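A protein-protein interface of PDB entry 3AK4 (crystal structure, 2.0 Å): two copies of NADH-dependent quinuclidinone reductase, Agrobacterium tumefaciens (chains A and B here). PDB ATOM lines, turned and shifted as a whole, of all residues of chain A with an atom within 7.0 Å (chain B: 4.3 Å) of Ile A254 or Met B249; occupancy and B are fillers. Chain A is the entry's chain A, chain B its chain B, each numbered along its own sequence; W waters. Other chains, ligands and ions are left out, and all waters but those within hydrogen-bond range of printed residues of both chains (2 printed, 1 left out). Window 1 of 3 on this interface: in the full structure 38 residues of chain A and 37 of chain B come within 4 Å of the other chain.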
ATOM      1  N   LYS A 150     -20.913   3.608 -36.618  1.00  0.00           N
ATOM      2  CA  LYS A 150     -19.450   3.563 -36.464  1.00  0.00           C
ATOM      3  C   LYS A 150     -18.762   3.059 -37.724  1.00  0.00           C
ATOM      4  O   LYS A 150     -17.648   3.499 -38.030  1.00  0.00           O
ATOM      5  CB  LYS A 150     -19.032   2.643 -35.283  1.00  0.00           C
ATOM      6  CG  LYS A 150     -19.509   3.139 -33.885  1.00  0.00           C
ATOM      7  CD  LYS A 150     -18.960   4.533 -33.563  1.00  0.00           C
ATOM      8  CE  LYS A 150     -19.357   5.019 -32.167  1.00  0.00           C
ATOM      9  NZ  LYS A 150     -18.692   4.239 -31.060  1.00  0.00           N
ATOM     10  N   PHE A 167     -25.488   9.954 -34.209  1.00  0.00           N
ATOM     11  CA  PHE A 167     -24.226  10.093 -33.469  1.00  0.00           C
ATOM     12  C   PHE A 167     -23.709  11.533 -33.576  1.00  0.00           C
ATOM     13  O   PHE A 167     -23.282  12.084 -32.568  1.00  0.00           O
ATOM     14  CB  PHE A 167     -23.183   9.066 -33.964  1.00  0.00           C
ATOM     15  CG  PHE A 167     -21.855   9.013 -33.149  1.00  0.00           C
ATOM     16  CD1 PHE A 167     -21.802   9.326 -31.774  1.00  0.00           C
ATOM     17  CD2 PHE A 167     -20.671   8.558 -33.778  1.00  0.00           C
ATOM     18  CE1 PHE A 167     -20.582   9.254 -31.059  1.00  0.00           C
ATOM     19  CE2 PHE A 167     -19.435   8.471 -33.062  1.00  0.00           C
ATOM     20  CZ  PHE A 167     -19.399   8.810 -31.704  1.00  0.00           C
ATOM     21  N   ASN A 185     -25.914  11.170 -24.525  1.00  0.00           N
ATOM     22  CA  ASN A 185     -25.056  10.080 -25.045  1.00  0.00           C
ATOM     23  C   ASN A 185     -25.832   9.174 -25.960  1.00  0.00           C
ATOM     24  O   ASN A 185     -27.065   9.230 -25.989  1.00  0.00           O
ATOM     25  CB  ASN A 185     -24.511   9.250 -23.866  1.00  0.00           C
ATOM     26  CG  ASN A 185     -23.529  10.035 -23.013  1.00  0.00           C
ATOM     27  OD1 ASN A 185     -22.416  10.330 -23.450  1.00  0.00           O
ATOM     28  ND2 ASN A 185     -23.944  10.393 -21.804  1.00  0.00           N
ATOM     29  N   CYS A 186     -25.153   8.283 -26.672  1.00  0.00           N
ATOM     30  CA  CYS A 186     -25.862   7.256 -27.435  1.00  0.00           C
ATOM     31  C   CYS A 186     -25.212   5.890 -27.217  1.00  0.00           C
ATOM     32  O   CYS A 186     -24.040   5.838 -26.783  1.00  0.00           O
ATOM     33  CB  CYS A 186     -25.987   7.619 -28.941  1.00  0.00           C
ATOM     34  SG  CYS A 186     -24.482   7.605 -29.922  1.00  0.00           S
ATOM     35  N   VAL A 187     -25.999   4.813 -27.425  1.00  0.00           N
ATOM     36  CA  VAL A 187     -25.507   3.423 -27.465  1.00  0.00           C
ATOM     37  C   VAL A 187     -25.516   2.917 -28.897  1.00  0.00           C
ATOM     38  O   VAL A 187     -26.396   3.301 -29.715  1.00  0.00           O
ATOM     39  CB  VAL A 187     -26.313   2.402 -26.543  1.00  0.00           C
ATOM     40  CG1 VAL A 187     -26.023   2.659 -25.102  1.00  0.00           C
ATOM     41  CG2 VAL A 187     -27.849   2.393 -26.849  1.00  0.00           C
ATOM     42  N   CYS A 188     -24.539   2.046 -29.187  1.00  0.00           N
ATOM     43  CA  CYS A 188     -24.336   1.503 -30.536  1.00  0.00           C
ATOM     44  C   CYS A 188     -24.410  -0.022 -30.412  1.00  0.00           C
ATOM     45  O   CYS A 188     -23.405  -0.673 -30.155  1.00  0.00           O
ATOM     46  CB  CYS A 188     -22.973   1.986 -31.108  1.00  0.00           C
ATOM     47  SG  CYS A 188     -22.945   3.808 -31.422  1.00  0.00           S
ATOM     48  N   PRO A 189     -25.635  -0.589 -30.473  1.00  0.00           N
ATOM     49  CA  PRO A 189     -25.762  -2.050 -30.335  1.00  0.00           C
ATOM     50  C   PRO A 189     -25.199  -2.859 -31.533  1.00  0.00           C
ATOM     51  O   PRO A 189     -25.066  -2.331 -32.622  1.00  0.00           O
ATOM     52  CB  PRO A 189     -27.290  -2.268 -30.198  1.00  0.00           C
ATOM     53  CG  PRO A 189     -27.855  -0.948 -29.858  1.00  0.00           C
ATOM     54  CD  PRO A 189     -26.952   0.064 -30.551  1.00  0.00           C
ATOM     55  N   LEU A 225     -17.143 -12.232 -28.359  1.00  0.00           N
ATOM     56  CA  LEU A 225     -17.726 -12.890 -27.196  1.00  0.00           C
ATOM     57  C   LEU A 225     -18.576 -14.141 -27.548  1.00  0.00           C
ATOM     58  O   LEU A 225     -19.050 -14.830 -26.647  1.00  0.00           O
ATOM     59  CB  LEU A 225     -18.494 -11.889 -26.315  1.00  0.00           C
ATOM     60  CG  LEU A 225     -17.659 -10.960 -25.441  1.00  0.00           C
ATOM     61  CD1 LEU A 225     -18.565  -9.929 -24.782  1.00  0.00           C
ATOM     62  CD2 LEU A 225     -16.885 -11.806 -24.372  1.00  0.00           C
ATOM     63  N   ASP A 233     -28.779  -6.944 -22.983  1.00  0.00           N
ATOM     64  CA  ASP A 233     -27.347  -6.542 -23.060  1.00  0.00           C
ATOM     65  C   ASP A 233     -27.213  -5.041 -23.302  1.00  0.00           C
ATOM     66  O   ASP A 233     -26.279  -4.382 -22.790  1.00  0.00           O
ATOM     67  CB  ASP A 233     -26.610  -7.298 -24.186  1.00  0.00           C
ATOM     68  CG  ASP A 233     -26.498  -8.812 -23.933  1.00  0.00           C
ATOM     69  OD1 ASP A 233     -26.155  -9.241 -22.803  1.00  0.00           O
ATOM     70  OD2 ASP A 233     -26.730  -9.582 -24.885  1.00  0.00           O
ATOM     71  N   VAL A 237     -26.769  -1.187 -20.134  1.00  0.00           N
ATOM     72  CA  VAL A 237     -25.820  -0.070 -20.415  1.00  0.00           C
ATOM     73  C   VAL A 237     -26.594   1.266 -20.476  1.00  0.00           C
ATOM     74  O   VAL A 237     -26.105   2.304 -20.005  1.00  0.00           O
ATOM     75  CB  VAL A 237     -24.944  -0.320 -21.706  1.00  0.00           C
ATOM     76  CG1 VAL A 237     -23.943   0.855 -21.954  1.00  0.00           C
ATOM     77  CG2 VAL A 237     -24.168  -1.664 -21.592  1.00  0.00           C
ATOM     78  N   PHE A 240     -26.992   2.457 -16.961  1.00  0.00           N
ATOM     79  CA  PHE A 240     -25.736   3.080 -16.529  1.00  0.00           C
ATOM     80  C   PHE A 240     -25.662   4.543 -16.993  1.00  0.00           C
ATOM     81  O   PHE A 240     -25.422   5.480 -16.174  1.00  0.00           O
ATOM     82  CB  PHE A 240     -24.533   2.300 -17.086  1.00  0.00           C
ATOM     83  CG  PHE A 240     -23.248   3.078 -17.033  1.00  0.00           C
ATOM     84  CD1 PHE A 240     -22.687   3.451 -15.798  1.00  0.00           C
ATOM     85  CD2 PHE A 240     -22.586   3.435 -18.218  1.00  0.00           C
ATOM     86  CE1 PHE A 240     -21.488   4.219 -15.754  1.00  0.00           C
ATOM     87  CE2 PHE A 240     -21.375   4.160 -18.172  1.00  0.00           C
ATOM     88  CZ  PHE A 240     -20.840   4.556 -16.940  1.00  0.00           C
ATOM     89  N   LEU A 241     -25.880   4.738 -18.294  1.00  0.00           N
ATOM     90  CA  LEU A 241     -25.760   6.081 -18.919  1.00  0.00           C
ATOM     91  C   LEU A 241     -26.788   7.075 -18.381  1.00  0.00           C
ATOM     92  O   LEU A 241     -26.517   8.258 -18.379  1.00  0.00           O
ATOM     93  CB  LEU A 241     -25.861   6.016 -20.468  1.00  0.00           C
ATOM     94  CG  LEU A 241     -24.661   5.343 -21.164  1.00  0.00           C
ATOM     95  CD1 LEU A 241     -24.915   5.097 -22.644  1.00  0.00           C
ATOM     96  CD2 LEU A 241     -23.344   6.167 -20.941  1.00  0.00           C
ATOM     97  N   MET A 249     -19.818  11.950 -18.096  1.00  0.00           N
ATOM     98  CA  MET A 249     -19.818  11.410 -19.478  1.00  0.00           C
ATOM     99  C   MET A 249     -20.914  12.036 -20.329  1.00  0.00           C
ATOM    100  O   MET A 249     -22.112  11.959 -19.994  1.00  0.00           O
ATOM    101  CB  MET A 249     -19.967   9.870 -19.497  1.00  0.00           C
ATOM    102  CG  MET A 249     -18.854   9.096 -18.797  1.00  0.00           C
ATOM    103  SD  MET A 249     -19.248   7.335 -18.747  1.00  0.00           S
ATOM    104  CE  MET A 249     -19.249   6.865 -20.486  1.00  0.00           C
ATOM    105  N   GLN A 252     -20.910  10.765 -25.958  1.00  0.00           N
ATOM    106  CA  GLN A 252     -20.299   9.465 -26.407  1.00  0.00           C
ATOM    107  C   GLN A 252     -21.205   8.571 -27.283  1.00  0.00           C
ATOM    108  O   GLN A 252     -22.445   8.685 -27.242  1.00  0.00           O
ATOM    109  CB  GLN A 252     -19.817   8.610 -25.225  1.00  0.00           C
ATOM    110  CG  GLN A 252     -18.991   9.302 -24.159  1.00  0.00           C
ATOM    111  CD  GLN A 252     -17.768  10.000 -24.736  1.00  0.00           C
ATOM    112  OE1 GLN A 252     -16.949   9.374 -25.425  1.00  0.00           O
ATOM    113  NE2 GLN A 252     -17.700  11.300 -24.552  1.00  0.00           N
ATOM    114  N   GLY A 253     -20.564   7.684 -28.056  1.00  0.00           N
ATOM    115  CA  GLY A 253     -21.181   6.533 -28.703  1.00  0.00           C
ATOM    116  C   GLY A 253     -20.659   5.245 -28.081  1.00  0.00           C
ATOM    117  O   GLY A 253     -19.676   4.641 -28.573  1.00  0.00           O
ATOM    118  N   ILE A 254     -21.335   4.801 -27.015  1.00  0.00           N
ATOM    119  CA  ILE A 254     -20.932   3.576 -26.295  1.00  0.00           C
ATOM    120  C   ILE A 254     -21.275   2.309 -27.089  1.00  0.00           C
ATOM    121  O   ILE A 254     -22.449   1.966 -27.333  1.00  0.00           O
ATOM    122  CB  ILE A 254     -21.447   3.528 -24.819  1.00  0.00           C
ATOM    123  CG1 ILE A 254     -21.119   4.859 -24.110  1.00  0.00           C
ATOM    124  CG2 ILE A 254     -20.865   2.287 -24.057  1.00  0.00           C
ATOM    125  CD1 ILE A 254     -19.581   5.152 -23.853  1.00  0.00           C
ATOM    126  N   ASN A 255     -20.214   1.615 -27.498  1.00  0.00           N
ATOM    127  CA  ASN A 255     -20.389   0.394 -28.257  1.00  0.00           C
ATOM    128  C   ASN A 255     -20.874  -0.717 -27.339  1.00  0.00           C
ATOM    129  O   ASN A 255     -20.318  -0.915 -26.252  1.00  0.00           O
ATOM    130  CB  ASN A 255     -19.067  -0.024 -28.938  1.00  0.00           C
ATOM    131  CG  ASN A 255     -18.597   0.965 -29.994  1.00  0.00           C
ATOM    132  OD1 ASN A 255     -19.398   1.560 -30.733  1.00  0.00           O
ATOM    133  ND2 ASN A 255     -17.275   1.156 -30.067  1.00  0.00           N
ATOM    134  N   VAL A 256     -21.914  -1.435 -27.766  1.00  0.00           N
ATOM    135  CA  VAL A 256     -22.369  -2.616 -27.019  1.00  0.00           C
ATOM    136  C   VAL A 256     -22.581  -3.750 -28.038  1.00  0.00           C
ATOM    137  O   VAL A 256     -23.711  -4.020 -28.472  1.00  0.00           O
ATOM    138  CB  VAL A 256     -23.654  -2.369 -26.096  1.00  0.00           C
ATOM    139  CG1 VAL A 256     -23.902  -3.593 -25.174  1.00  0.00           C
ATOM    140  CG2 VAL A 256     -23.521  -1.079 -25.213  1.00  0.00           C
ATOM    141  N   THR A 257     -21.478  -4.389 -28.424  1.00  0.00           N
ATOM    142  CA  THR A 257     -21.429  -5.282 -29.614  1.00  0.00           C
ATOM    143  C   THR A 257     -20.727  -6.620 -29.336  1.00  0.00           C
ATOM    144  O   THR A 257     -20.627  -7.477 -30.226  1.00  0.00           O
ATOM    145  CB  THR A 257     -20.698  -4.582 -30.843  1.00  0.00           C
ATOM    146  OG1 THR A 257     -19.309  -4.423 -30.541  1.00  0.00           O
ATOM    147  CG2 THR A 257     -21.269  -3.182 -31.096  1.00  0.00           C
ATOM    148  N   GLY A 258     -20.253  -6.807 -28.106  1.00  0.00           N
ATOM    149  CA  GLY A 258     -19.563  -8.053 -27.762  1.00  0.00           C
ATOM    150  C   GLY A 258     -18.182  -8.136 -28.400  1.00  0.00           C
ATOM    151  O   GLY A 258     -17.718  -9.236 -28.708  1.00  0.00           O
ATOM    152  N   GLY A 259     -17.548  -6.973 -28.585  1.00  0.00           N
ATOM    153  CA  GLY A 259     -16.186  -6.830 -29.153  1.00  0.00           C
ATOM    154  C   GLY A 259     -16.058  -6.631 -30.673  1.00  0.00           C
ATOM    155  O   GLY A 259     -14.939  -6.582 -31.202  1.00  0.00           O
ATOM    156  N   ARG B 183     -13.263 -10.542 -20.195  1.00  0.00           N
ATOM    157  CA  ARG B 183     -13.417  -9.166 -20.723  1.00  0.00           C
ATOM    158  C   ARG B 183     -12.269  -8.220 -20.328  1.00  0.00           C
ATOM    159  O   ARG B 183     -11.720  -8.297 -19.214  1.00  0.00           O
ATOM    160  CB  ARG B 183     -14.772  -8.549 -20.310  1.00  0.00           C
ATOM    161  CG  ARG B 183     -16.030  -9.347 -20.796  1.00  0.00           C
ATOM    162  CD  ARG B 183     -17.337  -8.581 -20.506  1.00  0.00           C
ATOM    163  NE  ARG B 183     -17.555  -8.296 -19.076  1.00  0.00           N
ATOM    164  CZ  ARG B 183     -17.392  -7.111 -18.490  1.00  0.00           C
ATOM    165  NH1 ARG B 183     -16.949  -6.045 -19.185  1.00  0.00           N
ATOM    166  NH2 ARG B 183     -17.655  -6.994 -17.182  1.00  0.00           N
ATOM    167  N   ASN B 185     -11.327  -4.089 -20.786  1.00  0.00           N
ATOM    168  CA  ASN B 185     -11.602  -2.704 -21.213  1.00  0.00           C
ATOM    169  C   ASN B 185     -10.627  -1.727 -20.579  1.00  0.00           C
ATOM    170  O   ASN B 185      -9.876  -2.088 -19.676  1.00  0.00           O
ATOM    171  CB  ASN B 185     -13.039  -2.314 -20.835  1.00  0.00           C
ATOM    172  CG  ASN B 185     -14.084  -3.104 -21.601  1.00  0.00           C
ATOM    173  OD1 ASN B 185     -14.266  -2.886 -22.786  1.00  0.00           O
ATOM    174  ND2 ASN B 185     -14.792  -4.026 -20.914  1.00  0.00           N
ATOM    175  N   PHE B 240     -18.857   0.087 -13.041  1.00  0.00           N
ATOM    176  CA  PHE B 240     -19.729  -0.365 -14.146  1.00  0.00           C
ATOM    177  C   PHE B 240     -19.020  -1.390 -15.077  1.00  0.00           C
ATOM    178  O   PHE B 240     -19.545  -2.475 -15.358  1.00  0.00           O
ATOM    179  CB  PHE B 240     -20.254   0.850 -14.954  1.00  0.00           C
ATOM    180  CG  PHE B 240     -20.785   0.469 -16.325  1.00  0.00           C
ATOM    181  CD1 PHE B 240     -22.011  -0.202 -16.453  1.00  0.00           C
ATOM    182  CD2 PHE B 240     -20.050   0.760 -17.467  1.00  0.00           C
ATOM    183  CE1 PHE B 240     -22.505  -0.576 -17.730  1.00  0.00           C
ATOM    184  CE2 PHE B 240     -20.512   0.402 -18.749  1.00  0.00           C
ATOM    185  CZ  PHE B 240     -21.739  -0.286 -18.880  1.00  0.00           C
ATOM    186  N   LEU B 241     -17.797  -1.071 -15.493  1.00  0.00           N
ATOM    187  CA  LEU B 241     -17.044  -1.916 -16.432  1.00  0.00           C
ATOM    188  C   LEU B 241     -16.664  -3.285 -15.829  1.00  0.00           C
ATOM    189  O   LEU B 241     -16.564  -4.296 -16.541  1.00  0.00           O
ATOM    190  CB  LEU B 241     -15.800  -1.145 -16.943  1.00  0.00           C
ATOM    191  CG  LEU B 241     -16.125   0.000 -17.925  1.00  0.00           C
ATOM    192  CD1 LEU B 241     -14.852   0.863 -18.309  1.00  0.00           C
ATOM    193  CD2 LEU B 241     -16.802  -0.559 -19.225  1.00  0.00           C
ATOM    194  N   ALA B 246     -21.930  -4.588 -17.822  1.00  0.00           N
ATOM    195  CA  ALA B 246     -21.014  -4.493 -18.941  1.00  0.00           C
ATOM    196  C   ALA B 246     -20.629  -5.863 -19.566  1.00  0.00           C
ATOM    197  O   ALA B 246     -19.649  -5.955 -20.292  1.00  0.00           O
ATOM    198  CB  ALA B 246     -19.740  -3.669 -18.538  1.00  0.00           C
ATOM    199  N   ARG B 247     -21.430  -6.911 -19.308  1.00  0.00           N
ATOM    200  CA  ARG B 247     -21.200  -8.256 -19.835  1.00  0.00           C
ATOM    201  C   ARG B 247     -21.039  -8.403 -21.371  1.00  0.00           C
ATOM    202  O   ARG B 247     -20.387  -9.361 -21.814  1.00  0.00           O
ATOM    203  CB  ARG B 247     -22.295  -9.213 -19.363  1.00  0.00           C
ATOM    204  CG  ARG B 247     -23.699  -8.967 -20.001  1.00  0.00           C
ATOM    205  CD  ARG B 247     -24.750  -9.735 -19.206  1.00  0.00           C
ATOM    206  NE  ARG B 247     -26.118  -9.416 -19.610  1.00  0.00           N
ATOM    207  CZ  ARG B 247     -26.819  -8.373 -19.170  1.00  0.00           C
ATOM    208  NH1 ARG B 247     -26.272  -7.520 -18.317  1.00  0.00           N
ATOM    209  NH2 ARG B 247     -28.079  -8.183 -19.589  1.00  0.00           N
ATOM    210  N   PHE B 248     -21.629  -7.497 -22.171  1.00  0.00           N
ATOM    211  CA  PHE B 248     -21.470  -7.577 -23.639  1.00  0.00           C
ATOM    212  C   PHE B 248     -20.537  -6.454 -24.183  1.00  0.00           C
ATOM    213  O   PHE B 248     -20.687  -5.986 -25.324  1.00  0.00           O
ATOM    214  CB  PHE B 248     -22.842  -7.614 -24.363  1.00  0.00           C
ATOM    215  CG  PHE B 248     -22.867  -8.505 -25.593  1.00  0.00           C
ATOM    216  CD1 PHE B 248     -22.680  -9.886 -25.475  1.00  0.00           C
ATOM    217  CD2 PHE B 248     -23.050  -7.972 -26.858  1.00  0.00           C
ATOM    218  CE1 PHE B 248     -22.698 -10.715 -26.609  1.00  0.00           C
ATOM    219  CE2 PHE B 248     -23.059  -8.817 -28.001  1.00  0.00           C
ATOM    220  CZ  PHE B 248     -22.874 -10.178 -27.861  1.00  0.00           C
ATOM    221  N   MET B 249     -19.563  -6.053 -23.366  1.00  0.00           N
ATOM    222  CA  MET B 249     -18.634  -4.964 -23.731  1.00  0.00           C
ATOM    223  C   MET B 249     -17.188  -5.361 -23.475  1.00  0.00           C
ATOM    224  O   MET B 249     -16.811  -5.646 -22.345  1.00  0.00           O
ATOM    225  CB  MET B 249     -18.924  -3.681 -22.932  1.00  0.00           C
ATOM    226  CG  MET B 249     -20.277  -2.976 -23.154  1.00  0.00           C
ATOM    227  SD  MET B 249     -20.479  -1.504 -22.068  1.00  0.00           S
ATOM    228  CE  MET B 249     -19.138  -0.422 -22.586  1.00  0.00           C
ATOM    229  N   THR B 250     -16.370  -5.346 -24.521  1.00  0.00           N
ATOM    230  CA  THR B 250     -14.941  -5.667 -24.375  1.00  0.00           C
ATOM    231  C   THR B 250     -14.051  -4.974 -25.420  1.00  0.00           C
ATOM    232  O   THR B 250     -14.505  -4.708 -26.538  1.00  0.00           O
ATOM    233  CB  THR B 250     -14.692  -7.216 -24.329  1.00  0.00           C
ATOM    234  OG1 THR B 250     -13.382  -7.452 -23.818  1.00  0.00           O
ATOM    235  CG2 THR B 250     -14.888  -7.911 -25.741  1.00  0.00           C
ATOM    236  N   ILE B 254     -13.262   3.729 -22.853  1.00  0.00           N
ATOM    237  CA  ILE B 254     -14.354   4.576 -22.379  1.00  0.00           C
ATOM    238  C   ILE B 254     -13.846   5.938 -21.886  1.00  0.00           C
ATOM    239  O   ILE B 254     -13.111   6.029 -20.881  1.00  0.00           O
ATOM    240  CB  ILE B 254     -15.222   3.866 -21.244  1.00  0.00           C
ATOM    241  CG1 ILE B 254     -15.651   2.445 -21.651  1.00  0.00           C
ATOM    242  CG2 ILE B 254     -16.443   4.725 -20.892  1.00  0.00           C
ATOM    243  CD1 ILE B 254     -16.689   2.315 -22.841  1.00  0.00           C
HETATM  244  O   HOH W   1     -28.302 -10.803 -21.702  1.00  0.00           O
HETATM  245  O   HOH W   2     -23.585  -5.218 -21.516  1.00  0.00           O
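Among the printed residues, merely in contact across the chains: Leu A225 with Arg B247 (3.5 Å), Leu A225 with Phe B248 (3.9 Å), Asp A233 with Phe B248 (3.8 Å), Val A237 with Phe B240 (3.9 Å), Val A237 with Met B249 (3.7 Å), Phe A240 with Phe B240 (3.6 Å), Met A249 with Ile B254 (3.6 Å), Ile A254 with Met B249 (3.5 Å), Asn A255 with Met B249 (3.7 Å), Val A256 with Phe B248 (3.99 Å), Thr A257 with Phe B248 (3.5 Å) and Gly A259 with Thr B250 (3.8 Å).
Water W1 bridges the side-chain carboxylate (OD1) of Asp A233 and the guanidinium group (NE) of Arg B247. Water W2 bridges the backbone NH (N) of Phe B248 and the backbone carbonyl oxygen (O) of Asp A233.
O of Met A249 lies within hydrogen-bond range of ND2 of Asn A185, 3.0 Å away. O of Cys A186 lies within hydrogen-bond range of N of Ile A254. N of Cys A188 is in hydrogen-bond range of O of Ile A254. The backbone NH (N) of Leu A225 is in hydrogen-bond range of the backbone carbonyl oxygen (O) of Gly A258 (3.1 Å). The backbone carbonyl oxygen (O) of Met B249 is in hydrogen-bond range of the guanidinium group (NH1) of Arg B183 (3.2 Å). The side-chain amide nitrogen (ND2) of Asn B185 sits at hydrogen-bond distance from the backbone carbonyl oxygen (O) of Met B249 (3.0 Å).
Ile A254 touches just one residue of chain B: Met B249. Of chain A, only Val A237, Ile A254 and Asn A255 come within 4 Å of Met B249. Of the printed residues of chain A, Phe B240 touches Val A237 (3.9 Å) and Phe A240 (3.6 Å). Printed residues of chain A within 4 Å of Arg B247: Leu A225 and Asp A233. Lys A150 touches none of the printed residues of chain B. Asn A185 touches none of the printed residues of chain B. The nearest residue of chain A that does not touch Met B249 is Val A256 (4.2 Å). The nearest printed residue of chain B that does not touch Thr A257 is Met B249 (5.5 Å).
Printed residues of chain B that touch a printed residue of chain A: Phe B240, Arg B247, Phe B248, Met B249, Thr B250 and Ile B254. Hydrophobic or aromatic side chains of chain B within 4 Å of the printed part of chain A: Phe B240, Phe B248, Met B249 and Ile B254. Printed residues of chain A that touch a printed residue of chain B: Leu A225, Asp A233, Val A237, Phe A240, Met A249, Ile A254, Asn A255, Val A256, Thr A257, Gly A258 and Gly A259.
Phe A240 touches its own counterpart, Phe B240. Met A249 touches Ile B254, and with the chains exchanged Ile A254 touches Met B249. Of the 14 pairs that touch across the chains among the printed residues, 3 have their exchanged pair printed and touching as well.
OD1 of Asp A233 is in salt-bridge range of NE of Arg B247, 3.2 Å away. N of Gly A258 lies within hydrogen-bond range of O of Phe B248 (2.9 Å).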
